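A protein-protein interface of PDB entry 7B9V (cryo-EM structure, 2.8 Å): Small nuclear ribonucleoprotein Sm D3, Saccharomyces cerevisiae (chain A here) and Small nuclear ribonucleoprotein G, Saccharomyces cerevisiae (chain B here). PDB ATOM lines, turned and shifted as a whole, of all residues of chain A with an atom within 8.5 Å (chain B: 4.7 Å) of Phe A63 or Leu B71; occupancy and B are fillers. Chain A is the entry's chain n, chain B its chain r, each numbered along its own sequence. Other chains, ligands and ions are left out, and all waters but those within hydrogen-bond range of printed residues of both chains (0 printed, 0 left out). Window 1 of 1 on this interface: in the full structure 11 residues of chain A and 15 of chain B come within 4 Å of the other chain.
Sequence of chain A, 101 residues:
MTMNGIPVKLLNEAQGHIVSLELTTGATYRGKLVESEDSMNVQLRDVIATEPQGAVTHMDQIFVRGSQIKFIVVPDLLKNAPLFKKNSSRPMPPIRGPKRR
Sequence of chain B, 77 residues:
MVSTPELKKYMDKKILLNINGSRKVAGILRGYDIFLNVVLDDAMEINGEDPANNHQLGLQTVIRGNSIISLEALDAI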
ATOM      1  N   LEU A  21      19.385 -27.344 -20.598  1.00  0.00           N
ATOM      2  CA  LEU A  21      18.281 -26.592 -21.172  1.00  0.00           C
ATOM      3  C   LEU A  21      18.731 -25.875 -22.430  1.00  0.00           C
ATOM      4  O   LEU A  21      19.807 -25.289 -22.444  1.00  0.00           O
ATOM      5  CB  LEU A  21      17.800 -25.553 -20.178  1.00  0.00           C
ATOM      6  CG  LEU A  21      16.517 -25.728 -19.413  1.00  0.00           C
ATOM      7  CD1 LEU A  21      16.641 -26.936 -18.493  1.00  0.00           C
ATOM      8  CD2 LEU A  21      16.393 -24.438 -18.662  1.00  0.00           C
ATOM      9  N   LEU A  23      16.990 -22.712 -24.837  1.00  0.00           N
ATOM     10  CA  LEU A  23      15.937 -21.714 -24.797  1.00  0.00           C
ATOM     11  C   LEU A  23      15.715 -21.152 -26.196  1.00  0.00           C
ATOM     12  O   LEU A  23      16.589 -21.252 -27.061  1.00  0.00           O
ATOM     13  CB  LEU A  23      16.316 -20.591 -23.821  1.00  0.00           C
ATOM     14  CG  LEU A  23      16.027 -20.741 -22.320  1.00  0.00           C
ATOM     15  CD1 LEU A  23      16.854 -21.803 -21.607  1.00  0.00           C
ATOM     16  CD2 LEU A  23      16.255 -19.400 -21.664  1.00  0.00           C
ATOM     17  N   TYR A  29      21.768 -23.719 -20.968  1.00  0.00           N
ATOM     18  CA  TYR A  29      22.112 -23.736 -19.549  1.00  0.00           C
ATOM     19  C   TYR A  29      22.212 -25.180 -19.080  1.00  0.00           C
ATOM     20  O   TYR A  29      21.225 -25.919 -19.143  1.00  0.00           O
ATOM     21  CB  TYR A  29      21.053 -22.973 -18.746  1.00  0.00           C
ATOM     22  CG  TYR A  29      20.956 -21.521 -19.149  1.00  0.00           C
ATOM     23  CD1 TYR A  29      21.760 -20.569 -18.550  1.00  0.00           C
ATOM     24  CD2 TYR A  29      20.092 -21.118 -20.159  1.00  0.00           C
ATOM     25  CE1 TYR A  29      21.645 -19.233 -18.895  1.00  0.00           C
ATOM     26  CE2 TYR A  29      20.014 -19.816 -20.550  1.00  0.00           C
ATOM     27  CZ  TYR A  29      20.782 -18.869 -19.914  1.00  0.00           C
ATOM     28  OH  TYR A  29      20.736 -17.568 -20.341  1.00  0.00           O
ATOM     29  N   GLU A  35      14.733 -27.374  -8.361  1.00  0.00           N
ATOM     30  CA  GLU A  35      13.288 -27.514  -8.301  1.00  0.00           C
ATOM     31  C   GLU A  35      12.704 -27.241  -9.678  1.00  0.00           C
ATOM     32  O   GLU A  35      13.211 -26.405 -10.428  1.00  0.00           O
ATOM     33  CB  GLU A  35      12.712 -26.551  -7.250  1.00  0.00           C
ATOM     34  CG  GLU A  35      11.206 -26.649  -7.000  1.00  0.00           C
ATOM     35  CD  GLU A  35      10.807 -26.381  -5.565  1.00  0.00           C
ATOM     36  OE1 GLU A  35      11.465 -25.559  -4.890  1.00  0.00           O
ATOM     37  OE2 GLU A  35       9.814 -26.993  -5.121  1.00  0.00           O
ATOM     38  N   SER A  36      11.638 -27.973 -10.001  1.00  0.00           N
ATOM     39  CA  SER A  36      10.890 -27.830 -11.235  1.00  0.00           C
ATOM     40  C   SER A  36       9.405 -27.751 -10.918  1.00  0.00           C
ATOM     41  O   SER A  36       8.938 -28.270  -9.900  1.00  0.00           O
ATOM     42  CB  SER A  36      11.147 -29.001 -12.183  1.00  0.00           C
ATOM     43  OG  SER A  36      10.763 -30.229 -11.587  1.00  0.00           O
ATOM     44  N   GLU A  37       8.672 -27.070 -11.790  1.00  0.00           N
ATOM     45  CA  GLU A  37       7.261 -26.779 -11.612  1.00  0.00           C
ATOM     46  C   GLU A  37       6.481 -27.330 -12.790  1.00  0.00           C
ATOM     47  O   GLU A  37       7.045 -27.527 -13.869  1.00  0.00           O
ATOM     48  CB  GLU A  37       7.056 -25.279 -11.585  1.00  0.00           C
ATOM     49  CG  GLU A  37       7.850 -24.589 -10.538  1.00  0.00           C
ATOM     50  CD  GLU A  37       7.658 -23.112 -10.606  1.00  0.00           C
ATOM     51  OE1 GLU A  37       6.628 -22.680 -11.157  1.00  0.00           O
ATOM     52  OE2 GLU A  37       8.556 -22.386 -10.145  1.00  0.00           O
ATOM     53  N   SER A  39       4.466 -26.056 -14.727  1.00  0.00           N
ATOM     54  CA  SER A  39       4.510 -25.124 -15.835  1.00  0.00           C
ATOM     55  C   SER A  39       5.772 -25.230 -16.691  1.00  0.00           C
ATOM     56  O   SER A  39       5.953 -24.377 -17.565  1.00  0.00           O
ATOM     57  CB  SER A  39       4.359 -23.713 -15.309  1.00  0.00           C
ATOM     58  OG  SER A  39       4.105 -22.879 -16.396  1.00  0.00           O
ATOM     59  N   MET A  40       6.661 -26.187 -16.398  1.00  0.00           N
ATOM     60  CA  MET A  40       8.053 -26.286 -16.875  1.00  0.00           C
ATOM     61  C   MET A  40       8.969 -25.129 -16.461  1.00  0.00           C
ATOM     62  O   MET A  40       9.994 -24.925 -17.104  1.00  0.00           O
ATOM     63  CB  MET A  40       8.150 -26.523 -18.391  1.00  0.00           C
ATOM     64  CG  MET A  40       7.430 -27.764 -18.860  1.00  0.00           C
ATOM     65  SD  MET A  40       7.528 -27.979 -20.643  1.00  0.00           S
ATOM     66  CE  MET A  40       9.245 -28.467 -20.823  1.00  0.00           C
ATOM     67  N   ASN A  41       8.657 -24.352 -15.421  1.00  0.00           N
ATOM     68  CA  ASN A  41       9.704 -23.518 -14.829  1.00  0.00           C
ATOM     69  C   ASN A  41      10.720 -24.429 -14.155  1.00  0.00           C
ATOM     70  O   ASN A  41      10.363 -25.448 -13.563  1.00  0.00           O
ATOM     71  CB  ASN A  41       9.152 -22.541 -13.794  1.00  0.00           C
ATOM     72  CG  ASN A  41       8.088 -21.621 -14.347  1.00  0.00           C
ATOM     73  OD1 ASN A  41       8.254 -21.032 -15.407  1.00  0.00           O
ATOM     74  ND2 ASN A  41       7.004 -21.475 -13.607  1.00  0.00           N
ATOM     75  N   VAL A  42      11.993 -24.043 -14.206  1.00  0.00           N
ATOM     76  CA  VAL A  42      13.059 -24.803 -13.554  1.00  0.00           C
ATOM     77  C   VAL A  42      14.051 -23.857 -12.891  1.00  0.00           C
ATOM     78  O   VAL A  42      14.233 -22.706 -13.300  1.00  0.00           O
ATOM     79  CB  VAL A  42      13.823 -25.772 -14.511  1.00  0.00           C
ATOM     80  CG1 VAL A  42      12.941 -26.892 -15.113  1.00  0.00           C
ATOM     81  CG2 VAL A  42      14.442 -25.007 -15.633  1.00  0.00           C
ATOM     82  N   GLN A  43      14.660 -24.361 -11.821  1.00  0.00           N
ATOM     83  CA  GLN A  43      15.780 -23.732 -11.134  1.00  0.00           C
ATOM     84  C   GLN A  43      17.052 -24.553 -11.305  1.00  0.00           C
ATOM     85  O   GLN A  43      17.084 -25.723 -10.913  1.00  0.00           O
ATOM     86  CB  GLN A  43      15.452 -23.647  -9.651  1.00  0.00           C
ATOM     87  CG  GLN A  43      14.156 -22.954  -9.343  1.00  0.00           C
ATOM     88  CD  GLN A  43      14.245 -22.162  -8.065  1.00  0.00           C
ATOM     89  OE1 GLN A  43      14.524 -20.969  -8.071  1.00  0.00           O
ATOM     90  NE2 GLN A  43      14.045 -22.846  -6.954  1.00  0.00           N
ATOM     91  N   LEU A  44      18.097 -23.950 -11.873  1.00  0.00           N
ATOM     92  CA  LEU A  44      19.374 -24.628 -12.054  1.00  0.00           C
ATOM     93  C   LEU A  44      20.461 -24.011 -11.180  1.00  0.00           C
ATOM     94  O   LEU A  44      20.519 -22.788 -11.027  1.00  0.00           O
ATOM     95  CB  LEU A  44      19.823 -24.586 -13.514  1.00  0.00           C
ATOM     96  CG  LEU A  44      18.889 -25.224 -14.531  1.00  0.00           C
ATOM     97  CD1 LEU A  44      19.488 -25.129 -15.926  1.00  0.00           C
ATOM     98  CD2 LEU A  44      18.666 -26.656 -14.121  1.00  0.00           C
ATOM     99  N   ARG A  45      21.300 -24.878 -10.590  1.00  0.00           N
ATOM    100  CA  ARG A  45      22.405 -24.526  -9.700  1.00  0.00           C
ATOM    101  C   ARG A  45      23.740 -24.933 -10.328  1.00  0.00           C
ATOM    102  O   ARG A  45      23.804 -25.950 -11.031  1.00  0.00           O
ATOM    103  CB  ARG A  45      22.221 -25.195  -8.323  1.00  0.00           C
ATOM    104  CG  ARG A  45      23.330 -25.133  -7.268  1.00  0.00           C
ATOM    105  CD  ARG A  45      22.856 -25.546  -5.909  1.00  0.00           C
ATOM    106  NE  ARG A  45      21.945 -24.532  -5.385  1.00  0.00           N
ATOM    107  CZ  ARG A  45      21.101 -24.727  -4.384  1.00  0.00           C
ATOM    108  NH1 ARG A  45      21.061 -25.879  -3.729  1.00  0.00           N
ATOM    109  NH2 ARG A  45      20.308 -23.729  -4.003  1.00  0.00           N
ATOM    110  N   VAL A  47      25.782 -23.466 -12.660  1.00  0.00           N
ATOM    111  CA  VAL A  47      25.300 -23.545 -14.030  1.00  0.00           C
ATOM    112  C   VAL A  47      26.384 -23.104 -14.992  1.00  0.00           C
ATOM    113  O   VAL A  47      27.022 -22.060 -14.800  1.00  0.00           O
ATOM    114  CB  VAL A  47      24.057 -22.660 -14.229  1.00  0.00           C
ATOM    115  CG1 VAL A  47      23.367 -22.969 -15.556  1.00  0.00           C
ATOM    116  CG2 VAL A  47      23.126 -22.826 -13.091  1.00  0.00           C
ATOM    117  N   MET A  59      27.524 -19.246 -13.879  1.00  0.00           N
ATOM    118  CA  MET A  59      26.737 -18.439 -12.947  1.00  0.00           C
ATOM    119  C   MET A  59      26.072 -19.308 -11.883  1.00  0.00           C
ATOM    120  O   MET A  59      25.739 -20.468 -12.133  1.00  0.00           O
ATOM    121  CB  MET A  59      25.692 -17.617 -13.717  1.00  0.00           C
ATOM    122  CG  MET A  59      24.755 -18.456 -14.577  1.00  0.00           C
ATOM    123  SD  MET A  59      23.590 -17.497 -15.564  1.00  0.00           S
ATOM    124  CE  MET A  59      24.707 -16.658 -16.686  1.00  0.00           C
ATOM    125  N   ASP A  60      25.938 -18.739 -10.665  1.00  0.00           N
ATOM    126  CA  ASP A  60      25.756 -19.525  -9.442  1.00  0.00           C
ATOM    127  C   ASP A  60      24.399 -20.227  -9.388  1.00  0.00           C
ATOM    128  O   ASP A  60      24.323 -21.401  -8.995  1.00  0.00           O
ATOM    129  CB  ASP A  60      25.886 -18.638  -8.198  1.00  0.00           C
ATOM    130  CG  ASP A  60      27.164 -17.824  -8.157  1.00  0.00           C
ATOM    131  OD1 ASP A  60      27.428 -17.080  -9.124  1.00  0.00           O
ATOM    132  OD2 ASP A  60      27.884 -17.897  -7.137  1.00  0.00           O
ATOM    133  N   GLN A  61      23.324 -19.535  -9.776  1.00  0.00           N
ATOM    134  CA  GLN A  61      21.980 -20.105  -9.820  1.00  0.00           C
ATOM    135  C   GLN A  61      21.154 -19.322 -10.845  1.00  0.00           C
ATOM    136  O   GLN A  61      21.389 -18.132 -11.053  1.00  0.00           O
ATOM    137  CB  GLN A  61      21.340 -20.091  -8.419  1.00  0.00           C
ATOM    138  CG  GLN A  61      20.013 -20.846  -8.297  1.00  0.00           C
ATOM    139  CD  GLN A  61      19.718 -21.290  -6.875  1.00  0.00           C
ATOM    140  OE1 GLN A  61      20.582 -21.805  -6.182  1.00  0.00           O
ATOM    141  NE2 GLN A  61      18.481 -21.083  -6.448  1.00  0.00           N
ATOM    142  N   ILE A  62      20.178 -19.987 -11.481  1.00  0.00           N
ATOM    143  CA  ILE A  62      19.252 -19.308 -12.390  1.00  0.00           C
ATOM    144  C   ILE A  62      17.870 -19.964 -12.298  1.00  0.00           C
ATOM    145  O   ILE A  62      17.745 -21.150 -11.985  1.00  0.00           O
ATOM    146  CB  ILE A  62      19.805 -19.295 -13.846  1.00  0.00           C
ATOM    147  CG1 ILE A  62      19.070 -18.285 -14.731  1.00  0.00           C
ATOM    148  CG2 ILE A  62      19.787 -20.674 -14.496  1.00  0.00           C
ATOM    149  CD1 ILE A  62      19.804 -17.931 -15.992  1.00  0.00           C
ATOM    150  N   PHE A  63      16.826 -19.148 -12.477  1.00  0.00           N
ATOM    151  CA  PHE A  63      15.439 -19.575 -12.667  1.00  0.00           C
ATOM    152  C   PHE A  63      15.004 -19.208 -14.085  1.00  0.00           C
ATOM    153  O   PHE A  63      15.168 -18.066 -14.509  1.00  0.00           O
ATOM    154  CB  PHE A  63      14.562 -18.925 -11.566  1.00  0.00           C
ATOM    155  CG  PHE A  63      13.029 -19.169 -11.650  1.00  0.00           C
ATOM    156  CD1 PHE A  63      12.205 -18.584 -12.625  1.00  0.00           C
ATOM    157  CD2 PHE A  63      12.439 -20.007 -10.725  1.00  0.00           C
ATOM    158  CE1 PHE A  63      10.878 -18.840 -12.675  1.00  0.00           C
ATOM    159  CE2 PHE A  63      11.074 -20.260 -10.772  1.00  0.00           C
ATOM    160  CZ  PHE A  63      10.297 -19.677 -11.747  1.00  0.00           C
ATOM    161  N   VAL A  64      14.438 -20.178 -14.813  1.00  0.00           N
ATOM    162  CA  VAL A  64      14.041 -20.008 -16.211  1.00  0.00           C
ATOM    163  C   VAL A  64      12.520 -20.155 -16.334  1.00  0.00           C
ATOM    164  O   VAL A  64      11.941 -21.109 -15.804  1.00  0.00           O
ATOM    165  CB  VAL A  64      14.756 -21.023 -17.123  1.00  0.00           C
ATOM    166  CG1 VAL A  64      14.357 -20.854 -18.592  1.00  0.00           C
ATOM    167  CG2 VAL A  64      16.259 -20.887 -16.990  1.00  0.00           C
ATOM    168  N   ARG A  65      11.883 -19.214 -17.040  1.00  0.00           N
ATOM    169  CA  ARG A  65      10.442 -19.242 -17.286  1.00  0.00           C
ATOM    170  C   ARG A  65      10.139 -20.311 -18.323  1.00  0.00           C
ATOM    171  O   ARG A  65      10.797 -20.344 -19.371  1.00  0.00           O
ATOM    172  CB  ARG A  65       9.924 -17.898 -17.780  1.00  0.00           C
ATOM    173  CG  ARG A  65       8.407 -17.870 -17.880  1.00  0.00           C
ATOM    174  CD  ARG A  65       7.908 -16.703 -18.711  1.00  0.00           C
ATOM    175  NE  ARG A  65       6.499 -16.834 -19.086  1.00  0.00           N
ATOM    176  CZ  ARG A  65       5.464 -16.607 -18.287  1.00  0.00           C
ATOM    177  NH1 ARG A  65       5.628 -16.218 -17.027  1.00  0.00           N
ATOM    178  NH2 ARG A  65       4.234 -16.779 -18.760  1.00  0.00           N
ATOM    179  N   GLY A  66       9.179 -21.209 -17.997  1.00  0.00           N
ATOM    180  CA  GLY A  66       8.870 -22.377 -18.830  1.00  0.00           C
ATOM    181  C   GLY A  66       8.600 -22.092 -20.299  1.00  0.00           C
ATOM    182  O   GLY A  66       9.017 -22.865 -21.169  1.00  0.00           O
ATOM    183  N   ILE A  69      11.642 -22.318 -22.619  1.00  0.00           N
ATOM    184  CA  ILE A  69      12.405 -23.545 -22.760  1.00  0.00           C
ATOM    185  C   ILE A  69      12.032 -24.226 -24.070  1.00  0.00           C
ATOM    186  O   ILE A  69      10.860 -24.484 -24.359  1.00  0.00           O
ATOM    187  CB  ILE A  69      12.196 -24.450 -21.541  1.00  0.00           C
ATOM    188  CG1 ILE A  69      12.777 -23.758 -20.313  1.00  0.00           C
ATOM    189  CG2 ILE A  69      12.869 -25.754 -21.746  1.00  0.00           C
ATOM    190  CD1 ILE A  69      12.619 -24.511 -19.030  1.00  0.00           C
ATOM    191  N   GLU B   6       8.374 -20.690  -7.564  1.00  0.00           N
ATOM    192  CA  GLU B   6       9.098 -20.919  -6.301  1.00  0.00           C
ATOM    193  C   GLU B   6      10.103 -19.833  -5.943  1.00  0.00           C
ATOM    194  O   GLU B   6      11.178 -20.102  -5.399  1.00  0.00           O
ATOM    195  CB  GLU B   6       9.753 -22.296  -6.318  1.00  0.00           C
ATOM    196  CG  GLU B   6       8.833 -23.446  -6.724  1.00  0.00           C
ATOM    197  CD  GLU B   6       7.403 -23.321  -6.165  1.00  0.00           C
ATOM    198  OE1 GLU B   6       7.246 -23.313  -4.919  1.00  0.00           O
ATOM    199  OE2 GLU B   6       6.450 -23.261  -6.962  1.00  0.00           O
ATOM    200  N   LEU B   7       9.760 -18.594  -6.275  1.00  0.00           N
ATOM    201  CA  LEU B   7      10.521 -17.372  -6.031  1.00  0.00           C
ATOM    202  C   LEU B   7      10.667 -17.009  -4.558  1.00  0.00           C
ATOM    203  O   LEU B   7      11.447 -16.095  -4.263  1.00  0.00           O
ATOM    204  CB  LEU B   7       9.910 -16.198  -6.816  1.00  0.00           C
ATOM    205  CG  LEU B   7      10.020 -15.983  -8.338  1.00  0.00           C
ATOM    206  CD1 LEU B   7      11.468 -15.845  -8.688  1.00  0.00           C
ATOM    207  CD2 LEU B   7       9.513 -17.100  -9.180  1.00  0.00           C
ATOM    208  N   TYR B  10      14.075 -16.562  -2.927  1.00  0.00           N
ATOM    209  CA  TYR B  10      14.886 -15.378  -3.171  1.00  0.00           C
ATOM    210  C   TYR B  10      14.564 -14.207  -2.255  1.00  0.00           C
ATOM    211  O   TYR B  10      15.510 -13.630  -1.695  1.00  0.00           O
ATOM    212  CB  TYR B  10      14.759 -14.973  -4.631  1.00  0.00           C
ATOM    213  CG  TYR B  10      15.218 -16.096  -5.507  1.00  0.00           C
ATOM    214  CD1 TYR B  10      16.460 -16.691  -5.295  1.00  0.00           C
ATOM    215  CD2 TYR B  10      14.409 -16.584  -6.519  1.00  0.00           C
ATOM    216  CE1 TYR B  10      16.902 -17.718  -6.106  1.00  0.00           C
ATOM    217  CE2 TYR B  10      14.827 -17.626  -7.318  1.00  0.00           C
ATOM    218  CZ  TYR B  10      16.082 -18.184  -7.112  1.00  0.00           C
ATOM    219  OH  TYR B  10      16.479 -19.248  -7.881  1.00  0.00           O
ATOM    220  N   ILE B  15      18.469  -9.695  -7.996  1.00  0.00           N
ATOM    221  CA  ILE B  15      18.194 -10.511  -9.168  1.00  0.00           C
ATOM    222  C   ILE B  15      18.630  -9.720 -10.392  1.00  0.00           C
ATOM    223  O   ILE B  15      18.412  -8.510 -10.422  1.00  0.00           O
ATOM    224  CB  ILE B  15      16.667 -10.744  -9.254  1.00  0.00           C
ATOM    225  CG1 ILE B  15      16.088 -11.387  -7.993  1.00  0.00           C
ATOM    226  CG2 ILE B  15      16.320 -11.665 -10.388  1.00  0.00           C
ATOM    227  CD1 ILE B  15      16.685 -12.664  -7.607  1.00  0.00           C
ATOM    228  N   LEU B  16      19.211 -10.372 -11.405  1.00  0.00           N
ATOM    229  CA  LEU B  16      19.196  -9.835 -12.769  1.00  0.00           C
ATOM    230  C   LEU B  16      18.198 -10.630 -13.598  1.00  0.00           C
ATOM    231  O   LEU B  16      18.214 -11.864 -13.589  1.00  0.00           O
ATOM    232  CB  LEU B  16      20.583  -9.791 -13.441  1.00  0.00           C
ATOM    233  CG  LEU B  16      20.690  -9.088 -14.825  1.00  0.00           C
ATOM    234  CD1 LEU B  16      22.057  -8.515 -14.972  1.00  0.00           C
ATOM    235  CD2 LEU B  16      20.541 -10.017 -16.043  1.00  0.00           C
ATOM    236  N   LEU B  17      17.338  -9.919 -14.318  1.00  0.00           N
ATOM    237  CA  LEU B  17      16.310 -10.499 -15.173  1.00  0.00           C
ATOM    238  C   LEU B  17      16.646 -10.213 -16.624  1.00  0.00           C
ATOM    239  O   LEU B  17      16.811  -9.055 -17.019  1.00  0.00           O
ATOM    240  CB  LEU B  17      14.922  -9.956 -14.842  1.00  0.00           C
ATOM    241  CG  LEU B  17      14.430 -10.341 -13.458  1.00  0.00           C
ATOM    242  CD1 LEU B  17      14.579  -9.151 -12.599  1.00  0.00           C
ATOM    243  CD2 LEU B  17      12.995 -10.727 -13.474  1.00  0.00           C
ATOM    244  N   LEU B  36       4.167 -14.994 -12.958  1.00  0.00           N
ATOM    245  CA  LEU B  36       5.458 -14.321 -12.757  1.00  0.00           C
ATOM    246  C   LEU B  36       5.499 -12.880 -13.200  1.00  0.00           C
ATOM    247  O   LEU B  36       6.553 -12.441 -13.663  1.00  0.00           O
ATOM    248  CB  LEU B  36       6.631 -15.047 -13.413  1.00  0.00           C
ATOM    249  CG  LEU B  36       6.770 -16.486 -13.007  1.00  0.00           C
ATOM    250  CD1 LEU B  36       8.005 -17.010 -13.652  1.00  0.00           C
ATOM    251  CD2 LEU B  36       6.882 -16.475 -11.541  1.00  0.00           C
ATOM    252  N   ILE B  68       9.557 -12.046 -19.001  1.00  0.00           N
ATOM    253  CA  ILE B  68      10.730 -12.589 -18.331  1.00  0.00           C
ATOM    254  C   ILE B  68      11.234 -13.767 -19.155  1.00  0.00           C
ATOM    255  O   ILE B  68      10.498 -14.719 -19.423  1.00  0.00           O
ATOM    256  CB  ILE B  68      10.379 -12.994 -16.889  1.00  0.00           C
ATOM    257  CG1 ILE B  68      10.240 -11.758 -16.003  1.00  0.00           C
ATOM    258  CG2 ILE B  68      11.418 -13.934 -16.309  1.00  0.00           C
ATOM    259  CD1 ILE B  68       9.751 -12.075 -14.602  1.00  0.00           C
ATOM    260  N   SER B  70      14.483 -15.343 -18.238  1.00  0.00           N
ATOM    261  CA  SER B  70      15.059 -16.052 -17.111  1.00  0.00           C
ATOM    262  C   SER B  70      15.615 -15.014 -16.151  1.00  0.00           C
ATOM    263  O   SER B  70      15.867 -13.866 -16.523  1.00  0.00           O
ATOM    264  CB  SER B  70      16.138 -17.036 -17.557  1.00  0.00           C
ATOM    265  OG  SER B  70      17.105 -16.388 -18.359  1.00  0.00           O
ATOM    266  N   LEU B  71      15.783 -15.429 -14.903  1.00  0.00           N
ATOM    267  CA  LEU B  71      16.296 -14.555 -13.866  1.00  0.00           C
ATOM    268  C   LEU B  71      17.346 -15.264 -13.024  1.00  0.00           C
ATOM    269  O   LEU B  71      17.157 -16.414 -12.612  1.00  0.00           O
ATOM    270  CB  LEU B  71      15.134 -14.035 -13.004  1.00  0.00           C
ATOM    271  CG  LEU B  71      14.270 -14.966 -12.136  1.00  0.00           C
ATOM    272  CD1 LEU B  71      14.626 -14.918 -10.661  1.00  0.00           C
ATOM    273  CD2 LEU B  71      12.795 -14.659 -12.341  1.00  0.00           C
ATOM    274  N   GLU B  72      18.488 -14.609 -12.841  1.00  0.00           N
ATOM    275  CA  GLU B  72      19.596 -15.157 -12.070  1.00  0.00           C
ATOM    276  C   GLU B  72      19.736 -14.387 -10.765  1.00  0.00           C
ATOM    277  O   GLU B  72      19.939 -13.167 -10.769  1.00  0.00           O
ATOM    278  CB  GLU B  72      20.891 -15.112 -12.889  1.00  0.00           C
ATOM    279  CG  GLU B  72      21.079 -13.850 -13.736  1.00  0.00           C
ATOM    280  CD  GLU B  72      22.521 -13.605 -14.139  1.00  0.00           C
ATOM    281  OE1 GLU B  72      23.429 -13.821 -13.309  1.00  0.00           O
ATOM    282  OE2 GLU B  72      22.739 -13.180 -15.293  1.00  0.00           O
ATOM    283  N   ALA B  73      19.587 -15.088  -9.645  1.00  0.00           N
ATOM    284  CA  ALA B  73      19.865 -14.482  -8.344  1.00  0.00           C
ATOM    285  C   ALA B  73      21.365 -14.349  -8.160  1.00  0.00           C
ATOM    286  O   ALA B  73      22.063 -15.325  -7.870  1.00  0.00           O
ATOM    287  CB  ALA B  73      19.278 -15.312  -7.210  1.00  0.00           C
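O of Phe A63 lies within hydrogen-bond range of N of Leu B71 (2.7 Å). The side-chain carboxylate (OE2) of Glu A37 sits at hydrogen-bond distance from the backbone NH (N) of Glu B6. The side-chain amide nitrogen (NE2) of Gln A61 lies within hydrogen-bond range of the side-chain hydroxyl (OH) of Tyr B10 (3.1 Å). OH of Tyr B10 lies within hydrogen-bond range of OE1 of Gln A43, 2.6 Å away.
The backbone carbonyl oxygen (O) of Leu B16 sits at hydrogen-bond distance from the backbone NH (N) of Glu B72, 2.9 Å away. OE1 of Glu A37 lies within hydrogen-bond range of ND2 of Asn A41. N of Leu A44 sits at hydrogen-bond distance from O of Ile A62 (2.8 Å). O of Glu A35 sits at hydrogen-bond distance from N of Gln A43 (2.9 Å). OE1 of Gln A61 is in hydrogen-bond range of NH2 of Arg A45 (2.9 Å). O of Val A42 sits at hydrogen-bond distance from N of Val A64.
Glu B6 touches Glu A35. O of Gln A61 touches CB of Glu B72 (3.6 Å). Gln A61 touches Ala B73. Ile A62 touches Ser B70. Leu B71 touches Ile A62. CZ of Phe A63 touches CD2 of Leu B7 (3.7 Å). Ser B70 touches Phe A63. Ser B70 touches Val A64 (CB to CA, 3.9 Å). Arg A65 touches Leu B36. O of Ile B68 touches CD of Arg A65, at 3.3 Å.
Phe A63 touches just these residues of chain B: Leu B7 (3.7 Å), Leu B36 (3.5 Å), Ser B70 (3.3 Å) and Leu B71 (2.7 Å). Of chain A, only Ile A62 and Phe A63 come within 4 Å of Leu B71. Ser B70 touches just these residues of chain A: Ile A62 (3.9 Å), Phe A63 (3.3 Å) and Val A64 (3.9 Å). Printed residues of chain A within 4 Å of Ala B73: Gln A61. Of the printed residues of chain A, Leu B7 touches Phe A63. Of the printed residues of chain B, Glu A35 touches Glu B6. Of the printed residues of chain A, Glu B6 touches Glu A35 and Glu A37. Of the printed residues of chain B, Glu A37 touches Glu B6. The nearest residue of chain A that does not touch Leu B71 is Gln A61 (4.8 Å).
Hydrophobic or aromatic side chains of chain B within 4 Å of the printed part of chain A: Leu B7, Tyr B10, Leu B36 and Leu B71. Printed residues of chain A that touch a printed residue of chain B: Glu A35, Glu A37, Gln A43, Gln A61, Ile A62, Phe A63, Val A64 and Arg A65. Along chain A the printed residues that touch a printed residue of chain B span positions 35 to 65. Among the printed residues, no Asp or Glu carboxylate lies within 4 Å of a Lys or Arg side-chain nitrogen of the other chain.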
